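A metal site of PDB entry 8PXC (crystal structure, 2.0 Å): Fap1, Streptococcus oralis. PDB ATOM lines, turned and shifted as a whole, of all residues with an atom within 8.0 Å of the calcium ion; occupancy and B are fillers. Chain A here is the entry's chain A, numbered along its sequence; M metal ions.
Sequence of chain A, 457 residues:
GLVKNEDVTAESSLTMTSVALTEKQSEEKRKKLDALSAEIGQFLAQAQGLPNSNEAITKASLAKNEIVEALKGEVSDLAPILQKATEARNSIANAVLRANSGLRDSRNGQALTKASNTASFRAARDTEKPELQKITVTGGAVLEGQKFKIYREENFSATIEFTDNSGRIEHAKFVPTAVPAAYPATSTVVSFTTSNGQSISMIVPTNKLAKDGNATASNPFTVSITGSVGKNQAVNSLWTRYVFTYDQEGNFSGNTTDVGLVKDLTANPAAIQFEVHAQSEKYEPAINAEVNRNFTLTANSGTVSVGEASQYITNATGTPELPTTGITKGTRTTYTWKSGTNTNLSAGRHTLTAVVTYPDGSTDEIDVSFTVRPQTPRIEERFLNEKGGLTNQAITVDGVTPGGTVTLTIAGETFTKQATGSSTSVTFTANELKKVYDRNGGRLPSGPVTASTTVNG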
ATOM      1  N   ARG A 125     -32.142  -5.225  19.431  1.00  0.00           N
ATOM      2  CA  ARG A 125     -32.297  -4.882  17.991  1.00  0.00           C
ATOM      3  C   ARG A 125     -30.933  -4.640  17.351  1.00  0.00           C
ATOM      4  O   ARG A 125     -29.961  -4.268  18.022  1.00  0.00           O
ATOM      5  CB  ARG A 125     -33.207  -3.667  17.786  1.00  0.00           C
ATOM      6  CG  ARG A 125     -34.529  -3.984  17.097  1.00  0.00           C
ATOM      7  CD  ARG A 125     -35.650  -3.171  17.707  1.00  0.00           C
ATOM      8  NE  ARG A 125     -35.288  -1.761  17.629  1.00  0.00           N
ATOM      9  CZ  ARG A 125     -35.797  -0.788  18.387  1.00  0.00           C
ATOM     10  NH1 ARG A 125     -36.702  -1.074  19.299  1.00  0.00           N
ATOM     11  NH2 ARG A 125     -35.387   0.454  18.224  1.00  0.00           N
ATOM     12  N   ASP A 126     -30.900  -4.907  16.045  1.00  0.00           N
ATOM     13  CA  ASP A 126     -29.725  -4.765  15.207  1.00  0.00           C
ATOM     14  C   ASP A 126     -29.379  -3.285  15.055  1.00  0.00           C
ATOM     15  O   ASP A 126     -30.136  -2.521  14.462  1.00  0.00           O
ATOM     16  CB  ASP A 126     -29.994  -5.382  13.844  1.00  0.00           C
ATOM     17  CG  ASP A 126     -28.831  -5.417  12.861  1.00  0.00           C
ATOM     18  OD1 ASP A 126     -27.753  -4.828  13.125  1.00  0.00           O
ATOM     19  OD2 ASP A 126     -29.029  -6.090  11.841  1.00  0.00           O
ATOM     20  N   THR A 127     -28.208  -2.901  15.561  1.00  0.00           N
ATOM     21  CA  THR A 127     -27.721  -1.539  15.385  1.00  0.00           C
ATOM     22  C   THR A 127     -26.345  -1.529  14.705  1.00  0.00           C
ATOM     23  O   THR A 127     -25.654  -0.521  14.758  1.00  0.00           O
ATOM     24  CB  THR A 127     -27.688  -0.767  16.704  1.00  0.00           C
ATOM     25  OG1 THR A 127     -26.710  -1.420  17.524  1.00  0.00           O
ATOM     26  CG2 THR A 127     -29.035  -0.710  17.400  1.00  0.00           C
ATOM     27  N   GLU A 128     -25.977  -2.628  14.040  1.00  0.00           N
ATOM     28  CA  GLU A 128     -24.673  -2.759  13.414  1.00  0.00           C
ATOM     29  C   GLU A 128     -24.810  -2.605  11.904  1.00  0.00           C
ATOM     30  O   GLU A 128     -25.615  -3.297  11.270  1.00  0.00           O
ATOM     31  CB  GLU A 128     -24.112  -4.136  13.764  1.00  0.00           C
ATOM     32  CG  GLU A 128     -22.738  -4.435  13.191  1.00  0.00           C
ATOM     33  CD  GLU A 128     -22.276  -5.857  13.496  1.00  0.00           C
ATOM     34  OE1 GLU A 128     -21.611  -6.468  12.623  1.00  0.00           O
ATOM     35  OE2 GLU A 128     -22.644  -6.352  14.614  1.00  0.00           O
ATOM     36  N   LYS A 129     -23.937  -1.776  11.316  1.00  0.00           N
ATOM     37  CA  LYS A 129     -23.915  -1.549   9.879  1.00  0.00           C
ATOM     38  C   LYS A 129     -23.485  -2.813   9.134  1.00  0.00           C
ATOM     39  O   LYS A 129     -22.554  -3.524   9.547  1.00  0.00           O
ATOM     40  CB  LYS A 129     -22.906  -0.467   9.505  1.00  0.00           C
ATOM     41  CG  LYS A 129     -23.212   0.927  10.052  1.00  0.00           C
ATOM     42  CD  LYS A 129     -22.131   1.909   9.602  1.00  0.00           C
ATOM     43  CE  LYS A 129     -22.451   3.379   9.868  1.00  0.00           C
ATOM     44  NZ  LYS A 129     -23.440   3.906   8.875  1.00  0.00           N
ATOM     45  N   PRO A 130     -24.063  -3.042   7.936  1.00  0.00           N
ATOM     46  CA  PRO A 130     -23.487  -4.012   7.003  1.00  0.00           C
ATOM     47  C   PRO A 130     -22.058  -3.578   6.653  1.00  0.00           C
ATOM     48  O   PRO A 130     -21.685  -2.411   6.764  1.00  0.00           O
ATOM     49  CB  PRO A 130     -24.357  -3.959   5.752  1.00  0.00           C
ATOM     50  CG  PRO A 130     -25.651  -3.322   6.226  1.00  0.00           C
ATOM     51  CD  PRO A 130     -25.300  -2.428   7.400  1.00  0.00           C
ATOM     52  N   GLU A 131     -21.233  -4.534   6.241  1.00  0.00           N
ATOM     53  CA  GLU A 131     -19.808  -4.319   6.092  1.00  0.00           C
ATOM     54  C   GLU A 131     -19.398  -4.775   4.703  1.00  0.00           C
ATOM     55  O   GLU A 131     -19.665  -5.918   4.297  1.00  0.00           O
ATOM     56  CB  GLU A 131     -19.060  -5.071   7.208  1.00  0.00           C
ATOM     57  CG  GLU A 131     -17.561  -4.971   7.117  1.00  0.00           C
ATOM     58  CD  GLU A 131     -16.971  -3.650   7.601  1.00  0.00           C
ATOM     59  OE1 GLU A 131     -17.770  -2.805   8.052  1.00  0.00           O
ATOM     60  OE2 GLU A 131     -15.717  -3.495   7.514  1.00  0.00           O
ATOM     61  N   THR A 163     -21.454  -8.293   3.915  1.00  0.00           N
ATOM     62  CA  THR A 163     -22.126  -9.078   4.951  1.00  0.00           C
ATOM     63  C   THR A 163     -22.828  -8.181   5.953  1.00  0.00           C
ATOM     64  O   THR A 163     -22.585  -6.972   6.026  1.00  0.00           O
ATOM     65  CB  THR A 163     -21.138  -9.982   5.685  1.00  0.00           C
ATOM     66  OG1 THR A 163     -20.179  -9.115   6.294  1.00  0.00           O
ATOM     67  CG2 THR A 163     -20.460 -10.955   4.742  1.00  0.00           C
ATOM     68  N   ASP A 164     -23.783  -8.789   6.674  1.00  0.00           N
ATOM     69  CA  ASP A 164     -24.403  -8.136   7.816  1.00  0.00           C
ATOM     70  C   ASP A 164     -24.516  -9.137   8.952  1.00  0.00           C
ATOM     71  O   ASP A 164     -24.689 -10.355   8.749  1.00  0.00           O
ATOM     72  CB  ASP A 164     -25.791  -7.580   7.503  1.00  0.00           C
ATOM     73  CG  ASP A 164     -26.298  -6.700   8.626  1.00  0.00           C
ATOM     74  OD1 ASP A 164     -25.712  -5.600   8.829  1.00  0.00           O
ATOM     75  OD2 ASP A 164     -27.268  -7.094   9.294  1.00  0.00           O
ATOM     76  N   ASN A 165     -24.449  -8.620  10.182  1.00  0.00           N
ATOM     77  CA  ASN A 165     -24.582  -9.447  11.366  1.00  0.00           C
ATOM     78  C   ASN A 165     -25.923 -10.189  11.407  1.00  0.00           C
ATOM     79  O   ASN A 165     -25.956 -11.277  11.936  1.00  0.00           O
ATOM     80  CB  ASN A 165     -24.365  -8.672  12.653  1.00  0.00           C
ATOM     81  CG  ASN A 165     -25.319  -7.513  12.797  1.00  0.00           C
ATOM     82  OD1 ASN A 165     -25.489  -6.709  11.914  1.00  0.00           O
ATOM     83  ND2 ASN A 165     -25.893  -7.359  13.969  1.00  0.00           N
ATOM     84  N   SER A 166     -26.986  -9.624  10.826  1.00  0.00           N
ATOM     85  CA  SER A 166     -28.282 -10.276  10.740  1.00  0.00           C
ATOM     86  C   SER A 166     -28.288 -11.398   9.702  1.00  0.00           C
ATOM     87  O   SER A 166     -29.218 -12.172   9.663  1.00  0.00           O
ATOM     88  CB  SER A 166     -29.373  -9.300  10.382  1.00  0.00           C
ATOM     89  OG  SER A 166     -29.220  -8.866   9.018  1.00  0.00           O
ATOM     90  N   GLY A 167     -27.324 -11.417   8.784  1.00  0.00           N
ATOM     91  CA  GLY A 167     -27.318 -12.341   7.663  1.00  0.00           C
ATOM     92  C   GLY A 167     -28.226 -11.870   6.526  1.00  0.00           C
ATOM     93  O   GLY A 167     -28.345 -12.585   5.537  1.00  0.00           O
ATOM     94  N   ARG A 168     -28.872 -10.688   6.643  1.00  0.00           N
ATOM     95  CA  ARG A 168     -29.836 -10.260   5.645  1.00  0.00           C
ATOM     96  C   ARG A 168     -29.624  -8.796   5.277  1.00  0.00           C
ATOM     97  O   ARG A 168     -29.591  -7.934   6.161  1.00  0.00           O
ATOM     98  CB  ARG A 168     -31.270 -10.483   6.154  1.00  0.00           C
ATOM     99  CG  ARG A 168     -32.341  -9.949   5.218  1.00  0.00           C
ATOM    100  CD  ARG A 168     -33.696 -10.542   5.517  1.00  0.00           C
ATOM    101  NE  ARG A 168     -34.798  -9.787   4.984  1.00  0.00           N
ATOM    102  CZ  ARG A 168     -36.067 -10.189   4.988  1.00  0.00           C
ATOM    103  NH1 ARG A 168     -36.384 -11.418   5.377  1.00  0.00           N
ATOM    104  NH2 ARG A 168     -37.004  -9.396   4.508  1.00  0.00           N
ATOM    105  N   ILE A 169     -29.514  -8.526   3.959  1.00  0.00           N
ATOM    106  CA  ILE A 169     -29.510  -7.162   3.449  1.00  0.00           C
ATOM    107  C   ILE A 169     -30.803  -6.947   2.646  1.00  0.00           C
ATOM    108  O   ILE A 169     -31.164  -7.794   1.828  1.00  0.00           O
ATOM    109  CB  ILE A 169     -28.213  -6.936   2.614  1.00  0.00           C
ATOM    110  CG1 ILE A 169     -27.021  -6.723   3.555  1.00  0.00           C
ATOM    111  CG2 ILE A 169     -28.393  -5.793   1.622  1.00  0.00           C
ATOM    112  CD1 ILE A 169     -25.648  -6.626   2.867  1.00  0.00           C
ATOM    113  N   TYR A 246     -28.196  -1.808   3.041  1.00  0.00           N
ATOM    114  CA  TYR A 246     -29.048  -1.593   4.201  1.00  0.00           C
ATOM    115  C   TYR A 246     -29.577  -2.908   4.740  1.00  0.00           C
ATOM    116  O   TYR A 246     -30.074  -3.711   3.945  1.00  0.00           O
ATOM    117  CB  TYR A 246     -30.245  -0.712   3.818  1.00  0.00           C
ATOM    118  CG  TYR A 246     -29.836   0.606   3.231  1.00  0.00           C
ATOM    119  CD1 TYR A 246     -29.503   0.691   1.902  1.00  0.00           C
ATOM    120  CD2 TYR A 246     -29.758   1.757   4.004  1.00  0.00           C
ATOM    121  CE1 TYR A 246     -29.109   1.884   1.328  1.00  0.00           C
ATOM    122  CE2 TYR A 246     -29.365   2.954   3.455  1.00  0.00           C
ATOM    123  CZ  TYR A 246     -29.011   3.027   2.113  1.00  0.00           C
ATOM    124  OH  TYR A 246     -28.564   4.177   1.515  1.00  0.00           O
ATOM    125  N   ASP A 247     -29.489  -3.108   6.063  1.00  0.00           N
ATOM    126  CA  ASP A 247     -30.178  -4.215   6.707  1.00  0.00           C
ATOM    127  C   ASP A 247     -31.648  -3.849   6.917  1.00  0.00           C
ATOM    128  O   ASP A 247     -32.077  -2.728   6.609  1.00  0.00           O
ATOM    129  CB  ASP A 247     -29.463  -4.648   7.989  1.00  0.00           C
ATOM    130  CG  ASP A 247     -29.448  -3.622   9.112  1.00  0.00           C
ATOM    131  OD1 ASP A 247     -30.296  -2.705   9.107  1.00  0.00           O
ATOM    132  OD2 ASP A 247     -28.545  -3.701   9.952  1.00  0.00           O
ATOM    133  N   GLN A 248     -32.413  -4.783   7.523  1.00  0.00           N
ATOM    134  CA  GLN A 248     -33.845  -4.550   7.705  1.00  0.00           C
ATOM    135  C   GLN A 248     -34.145  -3.395   8.651  1.00  0.00           C
ATOM    136  O   GLN A 248     -35.191  -2.781   8.481  1.00  0.00           O
ATOM    137  CB  GLN A 248     -34.561  -5.762   8.280  1.00  0.00           C
ATOM    138  CG  GLN A 248     -34.640  -6.912   7.312  1.00  0.00           C
ATOM    139  CD  GLN A 248     -34.954  -8.199   8.024  1.00  0.00           C
ATOM    140  OE1 GLN A 248     -36.106  -8.592   8.103  1.00  0.00           O
ATOM    141  NE2 GLN A 248     -33.922  -8.825   8.567  1.00  0.00           N
ATOM    142  N   GLU A 249     -33.257  -3.134   9.639  1.00  0.00           N
ATOM    143  CA  GLU A 249     -33.437  -2.053  10.578  1.00  0.00           C
ATOM    144  C   GLU A 249     -33.105  -0.701   9.956  1.00  0.00           C
ATOM    145  O   GLU A 249     -33.447   0.338  10.553  1.00  0.00           O
ATOM    146  CB  GLU A 249     -32.588  -2.244  11.844  1.00  0.00           C
ATOM    147  CG  GLU A 249     -33.101  -3.340  12.761  1.00  0.00           C
ATOM    148  CD  GLU A 249     -34.387  -3.000  13.497  1.00  0.00           C
ATOM    149  OE1 GLU A 249     -35.017  -3.929  14.019  1.00  0.00           O
ATOM    150  OE2 GLU A 249     -34.748  -1.827  13.561  1.00  0.00           O
ATOM    151  N   GLY A 250     -32.417  -0.703   8.801  1.00  0.00           N
ATOM    152  CA  GLY A 250     -32.094   0.556   8.160  1.00  0.00           C
ATOM    153  C   GLY A 250     -30.672   1.022   8.449  1.00  0.00           C
ATOM    154  O   GLY A 250     -30.287   2.099   7.978  1.00  0.00           O
ATOM    155  N   ASN A 251     -29.882   0.228   9.181  1.00  0.00           N
ATOM    156  CA  ASN A 251     -28.463   0.517   9.297  1.00  0.00           C
ATOM    157  C   ASN A 251     -27.827   0.372   7.921  1.00  0.00           C
ATOM    158  O   ASN A 251     -28.176  -0.550   7.189  1.00  0.00           O
ATOM    159  CB  ASN A 251     -27.738  -0.424  10.262  1.00  0.00           C
ATOM    160  CG  ASN A 251     -28.412  -0.493  11.605  1.00  0.00           C
ATOM    161  OD1 ASN A 251     -28.473   0.503  12.307  1.00  0.00           O
ATOM    162  ND2 ASN A 251     -28.973  -1.643  11.944  1.00  0.00           N
ATOM    163  N   PHE A 252     -26.871   1.255   7.593  1.00  0.00           N
ATOM    164  CA  PHE A 252     -26.284   1.303   6.248  1.00  0.00           C
ATOM    165  C   PHE A 252     -24.763   1.211   6.290  1.00  0.00           C
ATOM    166  O   PHE A 252     -24.133   1.751   7.193  1.00  0.00           O
ATOM    167  CB  PHE A 252     -26.710   2.560   5.498  1.00  0.00           C
ATOM    168  CG  PHE A 252     -26.349   3.860   6.150  1.00  0.00           C
ATOM    169  CD1 PHE A 252     -27.166   4.429   7.112  1.00  0.00           C
ATOM    170  CD2 PHE A 252     -25.188   4.533   5.808  1.00  0.00           C
ATOM    171  CE1 PHE A 252     -26.850   5.635   7.717  1.00  0.00           C
ATOM    172  CE2 PHE A 252     -24.863   5.743   6.409  1.00  0.00           C
ATOM    173  CZ  PHE A 252     -25.681   6.280   7.367  1.00  0.00           C
HETATM  174 CA    CA M   1     -27.017  -5.243  10.818  1.00  0.00          CA
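The side-chain carboxylate (OD1) of Asp 247 is in hydrogen-bond range of the backbone NH (N) of Asn 251, 3.0 Å away. OD1 of Asp 247 lies within hydrogen-bond range of N of Glu 249 (3.0 Å). The backbone NH of Gly 250 is in hydrogen-bond range of the side-chain carboxylate of Asp 247, at 2.9 Å. OD2 of Asp 164 sits close to OG of Ser 166 (2.7 Å). The backbone carbonyl oxygen of Asp 126 lies within hydrogen-bond range of the side-chain amide nitrogen of Asn 251.
Five residues have an atom within 4 Å of the calcium ion: Asp 126, Glu 128, Asp 164, Asn 165 and Asp 247. The nearest printed residue that does not touch the calcium ion is Asn 251 (4.2 Å).
The calcium ion is bound by OD2 of Asp 247 (2.3 Å), OD1 of Asn 165 (2.4 Å), OD1 of Asp 164 (2.4 Å), OD2 of Asp 126 (2.4 Å), OD2 of Asp 164 (2.4 Å), O of Glu 128 (2.4 Å) and OD1 of Asp 126 (2.5 Å).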
